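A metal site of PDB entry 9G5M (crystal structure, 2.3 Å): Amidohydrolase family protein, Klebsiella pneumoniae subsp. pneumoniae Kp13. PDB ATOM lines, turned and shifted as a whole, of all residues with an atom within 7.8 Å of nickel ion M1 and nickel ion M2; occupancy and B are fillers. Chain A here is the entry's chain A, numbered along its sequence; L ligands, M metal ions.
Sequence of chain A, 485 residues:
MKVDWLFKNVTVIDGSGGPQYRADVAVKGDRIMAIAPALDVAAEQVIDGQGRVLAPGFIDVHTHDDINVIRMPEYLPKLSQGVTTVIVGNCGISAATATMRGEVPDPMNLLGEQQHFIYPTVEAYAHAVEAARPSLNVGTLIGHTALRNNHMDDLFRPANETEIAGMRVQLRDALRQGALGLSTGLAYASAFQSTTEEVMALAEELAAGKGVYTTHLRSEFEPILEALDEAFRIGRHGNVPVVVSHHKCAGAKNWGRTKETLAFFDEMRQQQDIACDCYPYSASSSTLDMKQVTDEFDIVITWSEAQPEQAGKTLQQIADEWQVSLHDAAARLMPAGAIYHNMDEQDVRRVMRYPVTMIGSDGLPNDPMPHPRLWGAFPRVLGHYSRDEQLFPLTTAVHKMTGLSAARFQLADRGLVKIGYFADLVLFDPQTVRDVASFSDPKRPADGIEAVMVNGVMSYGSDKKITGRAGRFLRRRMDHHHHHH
Nickel ion M1 is bound by O4 of the ligand (2.1 Å), ND1 of His 216 (2.1 Å), NE2 of His 246 (2.2 Å) and SG of Cys 91 (2.3 Å).
Nickel ion M1 has four donor atoms within binding distance.
Nickel ion M2 is bound by a ring nitrogen (NE2) of His 64 (2.0 Å), an oxygen (O3) of the ligand (2.2 Å) and the side-chain sulfur of Cys 91 (2.4 Å).
Slightly farther from nickel ion M2 lies OD1 of Asp 362 (2.7 Å).
O of Cys 91 lies close to N of Gly 185, 3.5 Å away.
ND1 of His 246 is in hydrogen-bond range of OE2 of Glu 220, 3.0 Å away.
The backbone carbonyl oxygen (O) of His 62 is in hydrogen-bond range of the backbone NH (N) of Asp 362 (2.8 Å).
The side-chain carboxylate (OD1) of Asp 277 lies within hydrogen-bond range of the backbone NH (N) of His 246.
The backbone carbonyl oxygen (O) of His 216 lies within hydrogen-bond range of the backbone NH (N) of Leu 186, 3.2 Å away.
O of Thr 184 sits at hydrogen-bond distance from N of His 216 (2.8 Å).
The guanidinium group (NH2) of Arg 373 is in salt-bridge range of the side-chain carboxylate (OD2) of Asp 362 (3.3 Å).
The side-chain sulfur of Cys 91 sits close to a ring nitrogen (NE2) of His 62, at 3.3 Å.
Residues that only touch nickel ion M2: His 62 (2.1 Å).
Of the 28 residues printed, 4 come within 4 Å of nickel ion M2.
The nearest printed residue that does not touch nickel ion M2 is His 246 (4.01 Å).
Within 4 Å of nickel ion M1: Cys 91, His 216 and His 246.
Along chain A the residues within 4 Å of nickel ion M1 span positions 91 to 246.
The nearest printed residue that does not touch nickel ion M1 is His 62 (4.5 Å).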
ATOM      1  N   HIS A  62      14.694 -16.440 -11.221  1.00  0.00           N
ATOM      2  CA  HIS A  62      14.412 -16.093 -12.609  1.00  0.00           C
ATOM      3  C   HIS A  62      12.976 -16.457 -12.971  1.00  0.00           C
ATOM      4  O   HIS A  62      12.698 -17.582 -13.390  1.00  0.00           O
ATOM      5  CB  HIS A  62      15.407 -16.756 -13.538  1.00  0.00           C
ATOM      6  CG  HIS A  62      15.489 -16.098 -14.869  1.00  0.00           C
ATOM      7  ND1 HIS A  62      14.513 -16.253 -15.843  1.00  0.00           N
ATOM      8  CD2 HIS A  62      16.411 -15.263 -15.397  1.00  0.00           C
ATOM      9  CE1 HIS A  62      14.852 -15.555 -16.914  1.00  0.00           C
ATOM     10  NE2 HIS A  62      16.000 -14.954 -16.668  1.00  0.00           N
ATOM     11  N   THR A  63      12.072 -15.504 -12.831  1.00  0.00           N
ATOM     12  CA  THR A  63      10.679 -15.725 -13.163  1.00  0.00           C
ATOM     13  C   THR A  63      10.178 -14.614 -14.076  1.00  0.00           C
ATOM     14  O   THR A  63      10.762 -13.524 -14.167  1.00  0.00           O
ATOM     15  CB  THR A  63       9.756 -15.770 -11.930  1.00  0.00           C
ATOM     16  OG1 THR A  63       9.440 -14.436 -11.528  1.00  0.00           O
ATOM     17  CG2 THR A  63      10.437 -16.500 -10.759  1.00  0.00           C
ATOM     18  N   HIS A  64       9.072 -14.920 -14.737  1.00  0.00           N
ATOM     19  CA  HIS A  64       8.282 -13.943 -15.445  1.00  0.00           C
ATOM     20  C   HIS A  64       6.869 -13.940 -14.878  1.00  0.00           C
ATOM     21  O   HIS A  64       5.891 -13.915 -15.629  1.00  0.00           O
ATOM     22  CB  HIS A  64       8.337 -14.264 -16.945  1.00  0.00           C
ATOM     23  CG  HIS A  64       9.710 -14.148 -17.508  1.00  0.00           C
ATOM     24  ND1 HIS A  64      10.356 -12.928 -17.622  1.00  0.00           N
ATOM     25  CD2 HIS A  64      10.589 -15.089 -17.926  1.00  0.00           C
ATOM     26  CE1 HIS A  64      11.567 -13.134 -18.123  1.00  0.00           C
ATOM     27  NE2 HIS A  64      11.725 -14.425 -18.319  1.00  0.00           N
ATOM     28  N   GLY A  89      10.434  -9.614 -13.204  1.00  0.00           N
ATOM     29  CA  GLY A  89      11.021  -8.536 -13.979  1.00  0.00           C
ATOM     30  C   GLY A  89      12.320  -8.861 -14.665  1.00  0.00           C
ATOM     31  O   GLY A  89      13.210  -7.990 -14.757  1.00  0.00           O
ATOM     32  N   ASN A  90      12.472 -10.095 -15.157  1.00  0.00           N
ATOM     33  CA  ASN A  90      13.715 -10.567 -15.742  1.00  0.00           C
ATOM     34  C   ASN A  90      13.786 -10.320 -17.253  1.00  0.00           C
ATOM     35  O   ASN A  90      12.810  -9.917 -17.888  1.00  0.00           O
ATOM     36  CB  ASN A  90      13.914 -12.052 -15.436  1.00  0.00           C
ATOM     37  CG  ASN A  90      14.350 -12.270 -14.017  1.00  0.00           C
ATOM     38  OD1 ASN A  90      15.529 -12.178 -13.692  1.00  0.00           O
ATOM     39  ND2 ASN A  90      13.385 -12.512 -13.142  1.00  0.00           N
ATOM     40  N   CYS A  91      14.980 -10.562 -17.802  1.00  0.00           N
ATOM     41  CA  CYS A  91      15.257 -10.476 -19.245  1.00  0.00           C
ATOM     42  C   CYS A  91      14.840  -9.140 -19.851  1.00  0.00           C
ATOM     43  O   CYS A  91      14.421  -9.071 -21.012  1.00  0.00           O
ATOM     44  CB  CYS A  91      14.602 -11.626 -19.987  1.00  0.00           C
ATOM     45  SG  CYS A  91      15.151 -13.199 -19.326  1.00  0.00           S
ATOM     46  N   GLY A  92      14.966  -8.065 -19.093  1.00  0.00           N
ATOM     47  CA  GLY A  92      14.682  -6.746 -19.606  1.00  0.00           C
ATOM     48  C   GLY A  92      13.223  -6.342 -19.605  1.00  0.00           C
ATOM     49  O   GLY A  92      12.899  -5.237 -20.074  1.00  0.00           O
ATOM     50  N   ILE A  93      12.317  -7.185 -19.090  1.00  0.00           N
ATOM     51  CA  ILE A  93      10.882  -6.931 -19.155  1.00  0.00           C
ATOM     52  C   ILE A  93      10.299  -7.042 -17.753  1.00  0.00           C
ATOM     53  O   ILE A  93      10.450  -8.080 -17.084  1.00  0.00           O
ATOM     54  CB  ILE A  93      10.152  -7.887 -20.124  1.00  0.00           C
ATOM     55  CG1 ILE A  93      10.451  -9.362 -19.791  1.00  0.00           C
ATOM     56  CG2 ILE A  93      10.537  -7.561 -21.560  1.00  0.00           C
ATOM     57  CD1 ILE A  93       9.467 -10.334 -20.386  1.00  0.00           C
ATOM     58  N   PRO A 107       9.689  -8.695 -25.881  1.00  0.00           N
ATOM     59  CA  PRO A 107       8.792  -9.775 -25.443  1.00  0.00           C
ATOM     60  C   PRO A 107       7.965  -9.426 -24.205  1.00  0.00           C
ATOM     61  O   PRO A 107       7.653 -10.335 -23.429  1.00  0.00           O
ATOM     62  CB  PRO A 107       9.769 -10.900 -25.116  1.00  0.00           C
ATOM     63  CG  PRO A 107      10.941 -10.141 -24.485  1.00  0.00           C
ATOM     64  CD  PRO A 107      11.027  -8.825 -25.264  1.00  0.00           C
ATOM     65  N   LEU A 110       5.087 -11.635 -23.067  1.00  0.00           N
ATOM     66  CA  LEU A 110       5.183 -12.821 -22.210  1.00  0.00           C
ATOM     67  C   LEU A 110       4.452 -12.626 -20.892  1.00  0.00           C
ATOM     68  O   LEU A 110       3.978 -13.611 -20.301  1.00  0.00           O
ATOM     69  CB  LEU A 110       6.647 -13.172 -21.917  1.00  0.00           C
ATOM     70  CG  LEU A 110       7.546 -13.749 -23.023  1.00  0.00           C
ATOM     71  CD1 LEU A 110       8.923 -14.100 -22.453  1.00  0.00           C
ATOM     72  CD2 LEU A 110       6.920 -14.970 -23.643  1.00  0.00           C
ATOM     73  N   THR A 184      18.435  -7.012 -18.079  1.00  0.00           N
ATOM     74  CA  THR A 184      18.497  -6.757 -19.516  1.00  0.00           C
ATOM     75  C   THR A 184      18.142  -8.024 -20.279  1.00  0.00           C
ATOM     76  O   THR A 184      18.317  -9.145 -19.793  1.00  0.00           O
ATOM     77  CB  THR A 184      19.873  -6.256 -19.976  1.00  0.00           C
ATOM     78  OG1 THR A 184      20.883  -7.223 -19.643  1.00  0.00           O
ATOM     79  CG2 THR A 184      20.200  -4.910 -19.339  1.00  0.00           C
ATOM     80  N   GLY A 185      17.616  -7.820 -21.490  1.00  0.00           N
ATOM     81  CA  GLY A 185      17.395  -8.872 -22.449  1.00  0.00           C
ATOM     82  C   GLY A 185      17.910  -8.421 -23.793  1.00  0.00           C
ATOM     83  O   GLY A 185      17.124  -8.104 -24.701  1.00  0.00           O
ATOM     84  N   LEU A 186      19.234  -8.399 -23.929  1.00  0.00           N
ATOM     85  CA  LEU A 186      19.880  -7.705 -25.036  1.00  0.00           C
ATOM     86  C   LEU A 186      19.799  -8.479 -26.340  1.00  0.00           C
ATOM     87  O   LEU A 186      20.036  -7.888 -27.407  1.00  0.00           O
ATOM     88  CB  LEU A 186      21.343  -7.439 -24.659  1.00  0.00           C
ATOM     89  CG  LEU A 186      21.541  -6.589 -23.406  1.00  0.00           C
ATOM     90  CD1 LEU A 186      23.020  -6.458 -23.033  1.00  0.00           C
ATOM     91  CD2 LEU A 186      20.895  -5.208 -23.577  1.00  0.00           C
ATOM     92  N   ALA A 187      19.478  -9.768 -26.310  1.00  0.00           N
ATOM     93  CA  ALA A 187      19.330 -10.516 -27.553  1.00  0.00           C
ATOM     94  C   ALA A 187      18.017 -10.199 -28.267  1.00  0.00           C
ATOM     95  O   ALA A 187      17.917 -10.441 -29.466  1.00  0.00           O
ATOM     96  CB  ALA A 187      19.412 -12.017 -27.301  1.00  0.00           C
ATOM     97  N   TYR A 188      17.032  -9.651 -27.561  1.00  0.00           N
ATOM     98  CA  TYR A 188      15.749  -9.349 -28.180  1.00  0.00           C
ATOM     99  C   TYR A 188      15.853  -8.107 -29.058  1.00  0.00           C
ATOM    100  O   TYR A 188      16.536  -7.144 -28.724  1.00  0.00           O
ATOM    101  CB  TYR A 188      14.661  -9.145 -27.106  1.00  0.00           C
ATOM    102  CG  TYR A 188      14.286 -10.450 -26.469  1.00  0.00           C
ATOM    103  CD1 TYR A 188      13.449 -11.354 -27.120  1.00  0.00           C
ATOM    104  CD2 TYR A 188      14.776 -10.813 -25.210  1.00  0.00           C
ATOM    105  CE1 TYR A 188      13.101 -12.566 -26.539  1.00  0.00           C
ATOM    106  CE2 TYR A 188      14.430 -12.022 -24.621  1.00  0.00           C
ATOM    107  CZ  TYR A 188      13.597 -12.901 -25.290  1.00  0.00           C
ATOM    108  OH  TYR A 188      13.255 -14.122 -24.730  1.00  0.00           O
ATOM    109  N   THR A 215      21.322 -10.206 -16.514  1.00  0.00           N
ATOM    110  CA  THR A 215      21.350 -10.034 -17.960  1.00  0.00           C
ATOM    111  C   THR A 215      21.043 -11.338 -18.679  1.00  0.00           C
ATOM    112  O   THR A 215      21.707 -12.363 -18.474  1.00  0.00           O
ATOM    113  CB  THR A 215      22.690  -9.471 -18.421  1.00  0.00           C
ATOM    114  OG1 THR A 215      22.701  -9.445 -19.859  1.00  0.00           O
ATOM    115  CG2 THR A 215      23.867 -10.301 -17.911  1.00  0.00           C
ATOM    116  N   HIS A 216      20.029 -11.284 -19.517  1.00  0.00           N
ATOM    117  CA  HIS A 216      19.963 -12.153 -20.687  1.00  0.00           C
ATOM    118  C   HIS A 216      20.992 -11.616 -21.670  1.00  0.00           C
ATOM    119  O   HIS A 216      20.856 -10.496 -22.165  1.00  0.00           O
ATOM    120  CB  HIS A 216      18.553 -12.127 -21.244  1.00  0.00           C
ATOM    121  CG  HIS A 216      18.352 -12.971 -22.455  1.00  0.00           C
ATOM    122  ND1 HIS A 216      17.206 -13.700 -22.661  1.00  0.00           N
ATOM    123  CD2 HIS A 216      19.133 -13.180 -23.543  1.00  0.00           C
ATOM    124  CE1 HIS A 216      17.288 -14.337 -23.820  1.00  0.00           C
ATOM    125  NE2 HIS A 216      18.449 -14.040 -24.371  1.00  0.00           N
ATOM    126  N   LEU A 217      22.041 -12.395 -21.931  1.00  0.00           N
ATOM    127  CA  LEU A 217      23.175 -11.947 -22.739  1.00  0.00           C
ATOM    128  C   LEU A 217      22.752 -11.497 -24.137  1.00  0.00           C
ATOM    129  O   LEU A 217      21.770 -11.977 -24.695  1.00  0.00           O
ATOM    130  CB  LEU A 217      24.212 -13.064 -22.890  1.00  0.00           C
ATOM    131  CG  LEU A 217      24.924 -13.532 -21.638  1.00  0.00           C
ATOM    132  CD1 LEU A 217      25.856 -14.679 -22.024  1.00  0.00           C
ATOM    133  CD2 LEU A 217      25.707 -12.377 -20.958  1.00  0.00           C
ATOM    134  N   GLU A 220      23.515 -15.923 -26.786  1.00  0.00           N
ATOM    135  CA  GLU A 220      23.825 -17.189 -26.113  1.00  0.00           C
ATOM    136  C   GLU A 220      24.322 -18.242 -27.095  1.00  0.00           C
ATOM    137  O   GLU A 220      24.248 -19.446 -26.805  1.00  0.00           O
ATOM    138  CB  GLU A 220      22.599 -17.692 -25.331  1.00  0.00           C
ATOM    139  CG  GLU A 220      22.110 -16.736 -24.256  1.00  0.00           C
ATOM    140  CD  GLU A 220      21.163 -17.406 -23.260  1.00  0.00           C
ATOM    141  OE1 GLU A 220      20.145 -17.965 -23.699  1.00  0.00           O
ATOM    142  OE2 GLU A 220      21.450 -17.379 -22.035  1.00  0.00           O
ATOM    143  N   SER A 245      21.770 -14.481 -16.531  1.00  0.00           N
ATOM    144  CA  SER A 245      20.523 -15.222 -16.475  1.00  0.00           C
ATOM    145  C   SER A 245      20.576 -16.466 -17.349  1.00  0.00           C
ATOM    146  O   SER A 245      21.234 -16.500 -18.390  1.00  0.00           O
ATOM    147  CB  SER A 245      19.347 -14.339 -16.926  1.00  0.00           C
ATOM    148  OG  SER A 245      19.297 -13.126 -16.193  1.00  0.00           O
ATOM    149  N   HIS A 246      19.830 -17.485 -16.922  1.00  0.00           N
ATOM    150  CA  HIS A 246      19.720 -18.781 -17.592  1.00  0.00           C
ATOM    151  C   HIS A 246      20.937 -19.080 -18.462  1.00  0.00           C
ATOM    152  O   HIS A 246      20.822 -19.293 -19.677  1.00  0.00           O
ATOM    153  CB  HIS A 246      18.412 -18.861 -18.407  1.00  0.00           C
ATOM    154  CG  HIS A 246      18.161 -17.681 -19.313  1.00  0.00           C
ATOM    155  ND1 HIS A 246      19.028 -17.282 -20.291  1.00  0.00           N
ATOM    156  CD2 HIS A 246      17.087 -16.849 -19.396  1.00  0.00           C
ATOM    157  CE1 HIS A 246      18.523 -16.248 -20.943  1.00  0.00           C
ATOM    158  NE2 HIS A 246      17.346 -15.965 -20.421  1.00  0.00           N
ATOM    159  N   LYS A 248      23.547 -20.720 -20.598  1.00  0.00           N
ATOM    160  CA  LYS A 248      23.517 -21.901 -21.441  1.00  0.00           C
ATOM    161  C   LYS A 248      24.407 -21.644 -22.648  1.00  0.00           C
ATOM    162  O   LYS A 248      24.714 -20.490 -22.964  1.00  0.00           O
ATOM    163  CB  LYS A 248      22.088 -22.215 -21.929  1.00  0.00           C
ATOM    164  CG  LYS A 248      21.504 -21.091 -22.795  1.00  0.00           C
ATOM    165  CD  LYS A 248      20.187 -21.445 -23.446  1.00  0.00           C
ATOM    166  CE  LYS A 248      19.026 -21.381 -22.472  1.00  0.00           C
ATOM    167  NZ  LYS A 248      18.836 -19.983 -21.969  1.00  0.00           N
ATOM    168  N   ASP A 277      22.494 -17.880 -13.035  1.00  0.00           N
ATOM    169  CA  ASP A 277      21.495 -18.914 -12.739  1.00  0.00           C
ATOM    170  C   ASP A 277      21.259 -19.747 -13.999  1.00  0.00           C
ATOM    171  O   ASP A 277      21.700 -19.394 -15.091  1.00  0.00           O
ATOM    172  CB  ASP A 277      20.182 -18.320 -12.220  1.00  0.00           C
ATOM    173  CG  ASP A 277      19.552 -17.316 -13.177  1.00  0.00           C
ATOM    174  OD1 ASP A 277      18.950 -17.732 -14.196  1.00  0.00           O
ATOM    175  OD2 ASP A 277      19.664 -16.106 -12.920  1.00  0.00           O
ATOM    176  N   SER A 361      13.751 -21.071 -12.473  1.00  0.00           N
ATOM    177  CA  SER A 361      12.915 -21.899 -13.330  1.00  0.00           C
ATOM    178  C   SER A 361      12.788 -21.318 -14.730  1.00  0.00           C
ATOM    179  O   SER A 361      12.656 -22.070 -15.707  1.00  0.00           O
ATOM    180  CB  SER A 361      11.524 -22.065 -12.736  1.00  0.00           C
ATOM    181  OG  SER A 361      10.812 -20.827 -12.804  1.00  0.00           O
ATOM    182  N   ASP A 362      12.835 -19.992 -14.848  1.00  0.00           N
ATOM    183  CA  ASP A 362      12.538 -19.336 -16.115  1.00  0.00           C
ATOM    184  C   ASP A 362      11.205 -19.844 -16.660  1.00  0.00           C
ATOM    185  O   ASP A 362      11.031 -20.008 -17.867  1.00  0.00           O
ATOM    186  CB  ASP A 362      13.668 -19.531 -17.137  1.00  0.00           C
ATOM    187  CG  ASP A 362      13.569 -18.536 -18.309  1.00  0.00           C
ATOM    188  OD1 ASP A 362      12.885 -17.506 -18.157  1.00  0.00           O
ATOM    189  OD2 ASP A 362      14.176 -18.792 -19.364  1.00  0.00           O
ATOM    190  N   GLY A 363      10.259 -20.071 -15.761  1.00  0.00           N
ATOM    191  CA  GLY A 363       8.940 -20.514 -16.179  1.00  0.00           C
ATOM    192  C   GLY A 363       8.179 -19.421 -16.910  1.00  0.00           C
ATOM    193  O   GLY A 363       8.270 -18.239 -16.595  1.00  0.00           O
ATOM    194  N   LEU A 364       7.393 -19.839 -17.897  1.00  0.00           N
ATOM    195  CA  LEU A 364       6.566 -18.953 -18.697  1.00  0.00           C
ATOM    196  C   LEU A 364       5.102 -19.282 -18.443  1.00  0.00           C
ATOM    197  O   LEU A 364       4.556 -20.213 -19.054  1.00  0.00           O
ATOM    198  CB  LEU A 364       6.903 -19.084 -20.192  1.00  0.00           C
ATOM    199  CG  LEU A 364       8.369 -18.810 -20.537  1.00  0.00           C
ATOM    200  CD1 LEU A 364       8.587 -18.756 -22.042  1.00  0.00           C
ATOM    201  CD2 LEU A 364       8.860 -17.520 -19.898  1.00  0.00           C
ATOM    202  N   ARG A 373       9.736 -26.846 -16.623  1.00  0.00           N
ATOM    203  CA  ARG A 373      10.483 -26.125 -15.605  1.00  0.00           C
ATOM    204  C   ARG A 373       9.567 -25.217 -14.792  1.00  0.00           C
ATOM    205  O   ARG A 373       9.859 -24.902 -13.638  1.00  0.00           O
ATOM    206  CB  ARG A 373      11.601 -25.313 -16.256  1.00  0.00           C
ATOM    207  CG  ARG A 373      11.090 -24.222 -17.203  1.00  0.00           C
ATOM    208  CD  ARG A 373      12.208 -23.743 -18.113  1.00  0.00           C
ATOM    209  NE  ARG A 373      11.852 -22.491 -18.793  1.00  0.00           N
ATOM    210  CZ  ARG A 373      12.327 -22.150 -19.985  1.00  0.00           C
ATOM    211  NH1 ARG A 373      13.144 -22.947 -20.671  1.00  0.00           N
ATOM    212  NH2 ARG A 373      11.982 -20.975 -20.514  1.00  0.00           N
HETATM  213  S1  LIG L   1      13.209 -15.544 -21.781  1.00  0.00           S
HETATM  214  O1  LIG L   1      12.479 -16.572 -22.620  1.00  0.00           O
HETATM  215  O2  LIG L   1      12.428 -14.266 -21.749  1.00  0.00           O
HETATM  216  O3  LIG L   1      13.411 -16.136 -20.427  1.00  0.00           O
HETATM  217  O4  LIG L   1      14.518 -15.212 -22.387  1.00  0.00           O
HETATM  218 NI    NI M   1      15.942 -14.451 -21.095  1.00  0.00          NI
HETATM  219 NI    NI M   2      13.646 -14.969 -18.552  1.00  0.00          NI
